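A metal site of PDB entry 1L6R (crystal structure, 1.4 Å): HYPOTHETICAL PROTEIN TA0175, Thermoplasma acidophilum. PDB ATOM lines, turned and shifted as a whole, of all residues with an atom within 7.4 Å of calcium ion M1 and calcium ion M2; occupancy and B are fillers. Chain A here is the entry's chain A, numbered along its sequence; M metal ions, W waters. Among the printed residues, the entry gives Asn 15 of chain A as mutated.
OD1 of Asp 181 is in salt-bridge range of NZ of Lys 154 (2.8 Å). The side-chain amide nitrogen (ND2) of Asn 15 lies close to the backbone carbonyl oxygen (O) of Asp 11 (3.5 Å). ND2 of Asn 180 is in hydrogen-bond range of O of Tyr 140. The side-chain carboxylate of Asp 177 lies close to the side-chain hydroxyl of Ser 178, 3.2 Å away. The side-chain amide nitrogen (ND2) of Asn 180 lies within hydrogen-bond range of the side-chain hydroxyl (OG) of Ser 141 (3.5 Å). OD1 of Asn 180 lies close to OG of Ser 178 (3.2 Å). N of Ser 178 sits close to OD2 of Asp 181, at 2.9 Å. The backbone NH of Gly 14 sits at hydrogen-bond distance from the side-chain carboxylate of Asp 11.
Two residues have an atom within 4 Å of calcium ion M2: Gly 14 and Asp 177. The nearest printed residue that does not touch calcium ion M2 is Asn 196 (4.5 Å).
OD1 of Asn 180 binds calcium ion M1. OD2 of Asp 11 is bound to calcium ion M1 (2.4 Å). OD2 of Asp 181 is bound to calcium ion M1, 2.4 Å away. Calcium ion M1 is bound by the side-chain carboxylate (OD1) of Asp 177, at 2.4 Å. Water W3 binds calcium ion M1 (2.5 Å). Water W2 binds calcium ion M1 (2.7 Å). Slightly farther from calcium ion M1 lies OD1 of Asp 181 (2.9 Å). Slightly farther from calcium ion M1 lies OG of Ser 178 (3.1 Å).
OD2 of Asp 177 is bound to calcium ion M2, at 2.4 Å. Water W6 is bound to calcium ion M2, 2.5 Å away. Water W7 is bound to calcium ion M2 (2.5 Å). Water W4 binds calcium ion M2, 2.5 Å away. Water W5 binds calcium ion M2, 2.5 Å away. O of Gly 14 is bound to calcium ion M2, 2.6 Å away. Water W1 is bound to calcium ion M2 (2.6 Å).
Water W3 lies within hydrogen-bond range of OD1 of Asp 13 (3.0 Å), ND2 of Asn 180 (3.1 Å) and OG of Ser 178 (3.4 Å). Water W2 lies within hydrogen-bond range of OG of Ser 141 (2.9 Å), OD1 of Asp 11 (2.9 Å), NZ of Lys 154 (3.0 Å), OD1 of Asp 13 (3.4 Å) and ND2 of Asn 180 (3.5 Å). Water W1 bridges O of Asp 13 (2.6 Å) and OG1 of Thr 17 (3.4 Å).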
ATOM      1  N   ASP A  11      -6.539 -14.947  26.220  1.00  0.00           N
ATOM      2  CA  ASP A  11      -5.137 -14.503  26.158  1.00  0.00           C
ATOM      3  C   ASP A  11      -4.725 -14.204  27.602  1.00  0.00           C
ATOM      4  O   ASP A  11      -5.205 -13.253  28.223  1.00  0.00           O
ATOM      5  CB  ASP A  11      -5.089 -13.241  25.290  1.00  0.00           C
ATOM      6  CG  ASP A  11      -3.776 -12.521  25.368  1.00  0.00           C
ATOM      7  OD1 ASP A  11      -2.773 -13.055  25.878  1.00  0.00           O
ATOM      8  OD2 ASP A  11      -3.783 -11.366  24.901  1.00  0.00           O
ATOM      9  N   VAL A  12      -3.842 -15.035  28.137  1.00  0.00           N
ATOM     10  CA  VAL A  12      -3.403 -14.888  29.528  1.00  0.00           C
ATOM     11  C   VAL A  12      -2.756 -13.547  29.861  1.00  0.00           C
ATOM     12  O   VAL A  12      -3.218 -12.804  30.727  1.00  0.00           O
ATOM     13  CB  VAL A  12      -2.395 -16.004  29.905  1.00  0.00           C
ATOM     14  CG1 VAL A  12      -1.799 -15.745  31.287  1.00  0.00           C
ATOM     15  CG2 VAL A  12      -3.095 -17.357  29.888  1.00  0.00           C
ATOM     16  N   ASP A  13      -1.660 -13.230  29.169  1.00  0.00           N
ATOM     17  CA  ASP A  13      -0.974 -11.990  29.465  1.00  0.00           C
ATOM     18  C   ASP A  13      -1.788 -10.758  29.095  1.00  0.00           C
ATOM     19  O   ASP A  13      -1.777  -9.769  29.825  1.00  0.00           O
ATOM     20  CB  ASP A  13       0.403 -11.929  28.771  1.00  0.00           C
ATOM     21  CG  ASP A  13       0.304 -11.717  27.260  1.00  0.00           C
ATOM     22  OD1 ASP A  13      -0.374 -10.771  26.817  1.00  0.00           O
ATOM     23  OD2 ASP A  13       0.940 -12.496  26.507  1.00  0.00           O
ATOM     24  N   GLY A  14      -2.519 -10.832  27.992  1.00  0.00           N
ATOM     25  CA  GLY A  14      -3.272  -9.678  27.579  1.00  0.00           C
ATOM     26  C   GLY A  14      -4.517  -9.351  28.383  1.00  0.00           C
ATOM     27  O   GLY A  14      -4.866  -8.181  28.499  1.00  0.00           O
ATOM     28  N   ASN A  15      -5.146 -10.357  28.981  1.00  0.00           N
ATOM     29  CA  ASN A  15      -6.432 -10.140  29.661  1.00  0.00           C
ATOM     30  C   ASN A  15      -6.598 -10.615  31.092  1.00  0.00           C
ATOM     31  O   ASN A  15      -7.594 -10.278  31.722  1.00  0.00           O
ATOM     32  CB  ASN A  15      -7.519 -10.805  28.822  1.00  0.00           C
ATOM     33  CG  ASN A  15      -7.640 -10.215  27.449  1.00  0.00           C
ATOM     34  OD1 ASN A  15      -8.303  -9.183  27.262  1.00  0.00           O
ATOM     35  ND2 ASN A  15      -6.974 -10.819  26.477  1.00  0.00           N
ATOM     36  N   LEU A  16      -5.661 -11.408  31.597  1.00  0.00           N
ATOM     37  CA  LEU A  16      -5.822 -11.923  32.961  1.00  0.00           C
ATOM     38  C   LEU A  16      -4.868 -11.317  33.955  1.00  0.00           C
ATOM     39  O   LEU A  16      -4.811 -11.753  35.095  1.00  0.00           O
ATOM     40  CB  LEU A  16      -5.646 -13.448  32.964  1.00  0.00           C
ATOM     41  CG  LEU A  16      -6.622 -14.238  32.082  1.00  0.00           C
ATOM     42  CD1 LEU A  16      -6.382 -15.730  32.251  1.00  0.00           C
ATOM     43  CD2 LEU A  16      -8.058 -13.894  32.475  1.00  0.00           C
ATOM     44  N   THR A  17      -4.139 -10.284  33.550  1.00  0.00           N
ATOM     45  CA  THR A  17      -3.163  -9.661  34.435  1.00  0.00           C
ATOM     46  C   THR A  17      -3.395  -8.183  34.687  1.00  0.00           C
ATOM     47  O   THR A  17      -4.084  -7.509  33.906  1.00  0.00           O
ATOM     48  CB  THR A  17      -1.728  -9.856  33.902  1.00  0.00           C
ATOM     49  OG1 THR A  17      -1.594  -9.199  32.621  1.00  0.00           O
ATOM     50  CG2 THR A  17      -1.417 -11.336  33.724  1.00  0.00           C
ATOM     51  N   ASP A  18      -2.844  -7.671  35.777  1.00  0.00           N
ATOM     52  CA  ASP A  18      -3.004  -6.250  36.074  1.00  0.00           C
ATOM     53  C   ASP A  18      -1.824  -5.463  35.531  1.00  0.00           C
ATOM     54  O   ASP A  18      -1.017  -5.992  34.775  1.00  0.00           O
ATOM     55  CB  ASP A  18      -3.174  -6.022  37.592  1.00  0.00           C
ATOM     56  CG  ASP A  18      -1.958  -6.400  38.412  1.00  0.00           C
ATOM     57  OD1 ASP A  18      -0.825  -6.487  37.874  1.00  0.00           O
ATOM     58  OD2 ASP A  18      -2.124  -6.584  39.638  1.00  0.00           O
ATOM     59  N   TYR A 140       5.920  -9.315  19.919  1.00  0.00           N
ATOM     60  CA  TYR A 140       6.062  -9.283  21.364  1.00  0.00           C
ATOM     61  C   TYR A 140       4.778  -9.694  22.060  1.00  0.00           C
ATOM     62  O   TYR A 140       3.673  -9.363  21.606  1.00  0.00           O
ATOM     63  CB  TYR A 140       6.458  -7.865  21.809  1.00  0.00           C
ATOM     64  CG  TYR A 140       6.824  -7.765  23.271  1.00  0.00           C
ATOM     65  CD1 TYR A 140       5.851  -7.600  24.253  1.00  0.00           C
ATOM     66  CD2 TYR A 140       8.158  -7.901  23.674  1.00  0.00           C
ATOM     67  CE1 TYR A 140       6.189  -7.571  25.602  1.00  0.00           C
ATOM     68  CE2 TYR A 140       8.501  -7.876  25.011  1.00  0.00           C
ATOM     69  CZ  TYR A 140       7.522  -7.719  25.970  1.00  0.00           C
ATOM     70  OH  TYR A 140       7.851  -7.710  27.299  1.00  0.00           O
ATOM     71  N   SER A 141       4.916 -10.443  23.148  1.00  0.00           N
ATOM     72  CA  SER A 141       3.764 -10.825  23.956  1.00  0.00           C
ATOM     73  C   SER A 141       4.232 -11.196  25.349  1.00  0.00           C
ATOM     74  O   SER A 141       5.194 -11.954  25.511  1.00  0.00           O
ATOM     75  CB  SER A 141       3.006 -12.013  23.356  1.00  0.00           C
ATOM     76  OG  SER A 141       1.803 -12.216  24.086  1.00  0.00           O
ATOM     77  N   GLY A 142       3.572 -10.648  26.364  1.00  0.00           N
ATOM     78  CA  GLY A 142       3.926 -10.998  27.715  1.00  0.00           C
ATOM     79  C   GLY A 142       5.269 -10.483  28.190  1.00  0.00           C
ATOM     80  O   GLY A 142       5.467  -9.283  28.363  1.00  0.00           O
ATOM     81  N   LYS A 154      -2.540 -17.972  17.563  1.00  0.00           N
ATOM     82  CA  LYS A 154      -3.777 -18.181  18.286  1.00  0.00           C
ATOM     83  C   LYS A 154      -4.897 -18.763  17.422  1.00  0.00           C
ATOM     84  O   LYS A 154      -5.773 -19.435  17.942  1.00  0.00           O
ATOM     85  CB  LYS A 154      -4.234 -16.890  18.982  1.00  0.00           C
ATOM     86  CG  LYS A 154      -3.271 -16.406  20.083  1.00  0.00           C
ATOM     87  CD  LYS A 154      -3.947 -15.395  21.013  1.00  0.00           C
ATOM     88  CE  LYS A 154      -3.020 -14.892  22.123  1.00  0.00           C
ATOM     89  NZ  LYS A 154      -1.997 -13.911  21.635  1.00  0.00           N
ATOM     90  N   ILE A 175     -11.210 -13.987  23.848  1.00  0.00           N
ATOM     91  CA  ILE A 175     -10.954 -12.752  24.574  1.00  0.00           C
ATOM     92  C   ILE A 175      -9.480 -12.420  24.367  1.00  0.00           C
ATOM     93  O   ILE A 175      -8.596 -13.254  24.665  1.00  0.00           O
ATOM     94  CB  ILE A 175     -11.269 -12.911  26.090  1.00  0.00           C
ATOM     95  CG1 ILE A 175     -12.736 -13.327  26.255  1.00  0.00           C
ATOM     96  CG2 ILE A 175     -10.985 -11.611  26.826  1.00  0.00           C
ATOM     97  CD1 ILE A 175     -13.161 -13.570  27.684  1.00  0.00           C
ATOM     98  N   GLY A 176      -9.229 -11.231  23.827  1.00  0.00           N
ATOM     99  CA  GLY A 176      -7.883 -10.773  23.525  1.00  0.00           C
ATOM    100  C   GLY A 176      -7.801  -9.278  23.708  1.00  0.00           C
ATOM    101  O   GLY A 176      -8.785  -8.656  24.139  1.00  0.00           O
ATOM    102  N   ASP A 177      -6.670  -8.669  23.357  1.00  0.00           N
ATOM    103  CA  ASP A 177      -6.520  -7.229  23.576  1.00  0.00           C
ATOM    104  C   ASP A 177      -5.718  -6.436  22.552  1.00  0.00           C
ATOM    105  O   ASP A 177      -5.781  -5.214  22.562  1.00  0.00           O
ATOM    106  CB  ASP A 177      -5.876  -7.005  24.962  1.00  0.00           C
ATOM    107  CG  ASP A 177      -4.412  -7.430  25.002  1.00  0.00           C
ATOM    108  OD1 ASP A 177      -4.031  -8.316  24.238  1.00  0.00           O
ATOM    109  OD2 ASP A 177      -3.626  -6.895  25.815  1.00  0.00           O
ATOM    110  N   SER A 178      -4.978  -7.106  21.679  1.00  0.00           N
ATOM    111  CA  SER A 178      -4.115  -6.382  20.758  1.00  0.00           C
ATOM    112  C   SER A 178      -3.861  -7.111  19.455  1.00  0.00           C
ATOM    113  O   SER A 178      -4.475  -8.130  19.166  1.00  0.00           O
ATOM    114  CB  SER A 178      -2.777  -6.099  21.462  1.00  0.00           C
ATOM    115  OG  SER A 178      -2.162  -7.309  21.842  1.00  0.00           O
ATOM    116  N   ASN A 179      -2.939  -6.579  18.661  1.00  0.00           N
ATOM    117  CA  ASN A 179      -2.652  -7.156  17.359  1.00  0.00           C
ATOM    118  C   ASN A 179      -2.244  -8.618  17.375  1.00  0.00           C
ATOM    119  O   ASN A 179      -2.617  -9.356  16.472  1.00  0.00           O
ATOM    120  CB  ASN A 179      -1.582  -6.324  16.630  1.00  0.00           C
ATOM    121  CG  ASN A 179      -1.200  -6.929  15.299  1.00  0.00           C
ATOM    122  OD1 ASN A 179      -0.186  -7.627  15.189  1.00  0.00           O
ATOM    123  ND2 ASN A 179      -2.007  -6.691  14.280  1.00  0.00           N
ATOM    124  N   ASN A 180      -1.504  -9.047  18.390  1.00  0.00           N
ATOM    125  CA  ASN A 180      -1.096 -10.441  18.430  1.00  0.00           C
ATOM    126  C   ASN A 180      -2.283 -11.385  18.689  1.00  0.00           C
ATOM    127  O   ASN A 180      -2.111 -12.602  18.751  1.00  0.00           O
ATOM    128  CB  ASN A 180       0.063 -10.678  19.438  1.00  0.00           C
ATOM    129  CG  ASN A 180      -0.287 -10.298  20.858  1.00  0.00           C
ATOM    130  OD1 ASN A 180      -1.447 -10.329  21.240  1.00  0.00           O
ATOM    131  ND2 ASN A 180       0.730  -9.970  21.668  1.00  0.00           N
ATOM    132  N   ASP A 181      -3.479 -10.830  18.815  1.00  0.00           N
ATOM    133  CA  ASP A 181      -4.698 -11.628  18.993  1.00  0.00           C
ATOM    134  C   ASP A 181      -5.578 -11.578  17.760  1.00  0.00           C
ATOM    135  O   ASP A 181      -6.561 -12.310  17.667  1.00  0.00           O
ATOM    136  CB  ASP A 181      -5.520 -11.136  20.153  1.00  0.00           C
ATOM    137  CG  ASP A 181      -4.720 -11.056  21.393  1.00  0.00           C
ATOM    138  OD1 ASP A 181      -4.158 -12.092  21.785  1.00  0.00           O
ATOM    139  OD2 ASP A 181      -4.650  -9.949  21.959  1.00  0.00           O
ATOM    140  N   MET A 182      -5.253 -10.708  16.810  1.00  0.00           N
ATOM    141  CA  MET A 182      -6.084 -10.613  15.618  1.00  0.00           C
ATOM    142  C   MET A 182      -6.259 -11.955  14.912  1.00  0.00           C
ATOM    143  O   MET A 182      -7.310 -12.197  14.336  1.00  0.00           O
ATOM    144  CB  MET A 182      -5.537  -9.553  14.653  1.00  0.00           C
ATOM    145  CG  MET A 182      -6.481  -9.254  13.475  1.00  0.00           C
ATOM    146  SD  MET A 182      -8.183  -8.794  13.938  1.00  0.00           S
ATOM    147  CE  MET A 182      -7.977  -7.017  14.272  1.00  0.00           C
ATOM    148  N   MET A 184      -7.010 -14.799  16.059  1.00  0.00           N
ATOM    149  CA  MET A 184      -8.216 -15.477  16.500  1.00  0.00           C
ATOM    150  C   MET A 184      -9.447 -14.570  16.371  1.00  0.00           C
ATOM    151  O   MET A 184     -10.552 -15.065  16.179  1.00  0.00           O
ATOM    152  CB  MET A 184      -8.074 -16.028  17.937  1.00  0.00           C
ATOM    153  CG  MET A 184      -7.883 -15.030  19.055  1.00  0.00           C
ATOM    154  SD  MET A 184      -7.752 -15.962  20.607  1.00  0.00           S
ATOM    155  CE  MET A 184      -7.568 -14.611  21.760  1.00  0.00           C
ATOM    156  N   PRO A 194     -11.229  -5.882  26.345  1.00  0.00           N
ATOM    157  CA  PRO A 194     -11.227  -4.881  27.419  1.00  0.00           C
ATOM    158  C   PRO A 194     -11.299  -3.437  26.901  1.00  0.00           C
ATOM    159  O   PRO A 194     -11.173  -3.165  25.699  1.00  0.00           O
ATOM    160  CB  PRO A 194      -9.919  -5.164  28.156  1.00  0.00           C
ATOM    161  CG  PRO A 194      -9.013  -5.639  27.037  1.00  0.00           C
ATOM    162  CD  PRO A 194      -9.906  -6.536  26.218  1.00  0.00           C
ATOM    163  N   ASN A 196      -9.164  -1.198  27.250  1.00  0.00           N
ATOM    164  CA  ASN A 196      -7.889  -0.717  26.716  1.00  0.00           C
ATOM    165  C   ASN A 196      -7.391  -1.562  25.544  1.00  0.00           C
ATOM    166  O   ASN A 196      -6.211  -1.550  25.194  1.00  0.00           O
ATOM    167  CB  ASN A 196      -6.831  -0.640  27.831  1.00  0.00           C
ATOM    168  CG  ASN A 196      -6.344  -1.994  28.279  1.00  0.00           C
ATOM    169  OD1 ASN A 196      -6.946  -3.019  27.972  1.00  0.00           O
ATOM    170  ND2 ASN A 196      -5.235  -2.008  29.016  1.00  0.00           N
ATOM    171  N   ALA A 197      -8.304  -2.303  24.922  1.00  0.00           N
ATOM    172  CA  ALA A 197      -7.926  -3.087  23.751  1.00  0.00           C
ATOM    173  C   ALA A 197      -7.634  -2.110  22.601  1.00  0.00           C
ATOM    174  O   ALA A 197      -8.077  -0.965  22.622  1.00  0.00           O
ATOM    175  CB  ALA A 197      -9.058  -4.018  23.345  1.00  0.00           C
ATOM    176  N   SER A 212     -10.721  -3.258  32.281  1.00  0.00           N
ATOM    177  CA  SER A 212      -9.480  -3.835  31.791  1.00  0.00           C
ATOM    178  C   SER A 212      -8.756  -4.459  32.981  1.00  0.00           C
ATOM    179  O   SER A 212      -9.254  -4.446  34.111  1.00  0.00           O
ATOM    180  CB  SER A 212      -8.558  -2.763  31.200  1.00  0.00           C
ATOM    181  OG  SER A 212      -9.197  -2.026  30.182  1.00  0.00           O
ATOM    182  N   TYR A 213      -7.571  -4.995  32.707  1.00  0.00           N
ATOM    183  CA  TYR A 213      -6.700  -5.602  33.716  1.00  0.00           C
ATOM    184  C   TYR A 213      -7.310  -6.753  34.503  1.00  0.00           C
ATOM    185  O   TYR A 213      -7.027  -6.942  35.693  1.00  0.00           O
ATOM    186  CB  TYR A 213      -6.182  -4.488  34.654  1.00  0.00           C
ATOM    187  CG  TYR A 213      -5.236  -3.525  33.940  1.00  0.00           C
ATOM    188  CD1 TYR A 213      -4.056  -3.975  33.358  1.00  0.00           C
ATOM    189  CD2 TYR A 213      -5.531  -2.157  33.876  1.00  0.00           C
ATOM    190  CE1 TYR A 213      -3.185  -3.093  32.722  1.00  0.00           C
ATOM    191  CE2 TYR A 213      -4.656  -1.266  33.240  1.00  0.00           C
ATOM    192  CZ  TYR A 213      -3.485  -1.744  32.668  1.00  0.00           C
ATOM    193  OH  TYR A 213      -2.627  -0.867  32.037  1.00  0.00           O
ATOM    194  N   GLU A 216     -12.407  -7.188  33.021  1.00  0.00           N
ATOM    195  CA  GLU A 216     -13.298  -7.341  31.868  1.00  0.00           C
ATOM    196  C   GLU A 216     -13.851  -8.759  31.813  1.00  0.00           C
ATOM    197  O   GLU A 216     -14.922  -8.991  31.238  1.00  0.00           O
ATOM    198  CB  GLU A 216     -12.561  -7.036  30.548  1.00  0.00           C
ATOM    199  CG  GLU A 216     -11.524  -8.068  30.106  1.00  0.00           C
ATOM    200  CD  GLU A 216     -10.128  -7.715  30.581  1.00  0.00           C
ATOM    201  OE1 GLU A 216      -9.982  -7.253  31.722  1.00  0.00           O
ATOM    202  OE2 GLU A 216      -9.167  -7.920  29.790  1.00  0.00           O
HETATM  203 CA    CA M   1      -2.642 -10.048  23.271  1.00  0.00          CA
HETATM  204 CA    CA M   2      -3.561  -6.039  28.035  1.00  0.00          CA
HETATM  205  O   HOH W   1      -2.599  -7.288  30.040  1.00  0.00           O
HETATM  206  O   HOH W   2      -1.030 -12.113  23.789  1.00  0.00           O
HETATM  207  O   HOH W   3      -0.605  -9.056  24.323  1.00  0.00           O
HETATM  208  O   HOH W   4      -1.070  -6.189  27.611  1.00  0.00           O
HETATM  209  O   HOH W   5      -3.025  -4.292  29.802  1.00  0.00           O
HETATM  210  O   HOH W   6      -5.889  -5.358  28.402  1.00  0.00           O
HETATM  211  O   HOH W   7      -3.403  -3.975  26.679  1.00  0.00           O
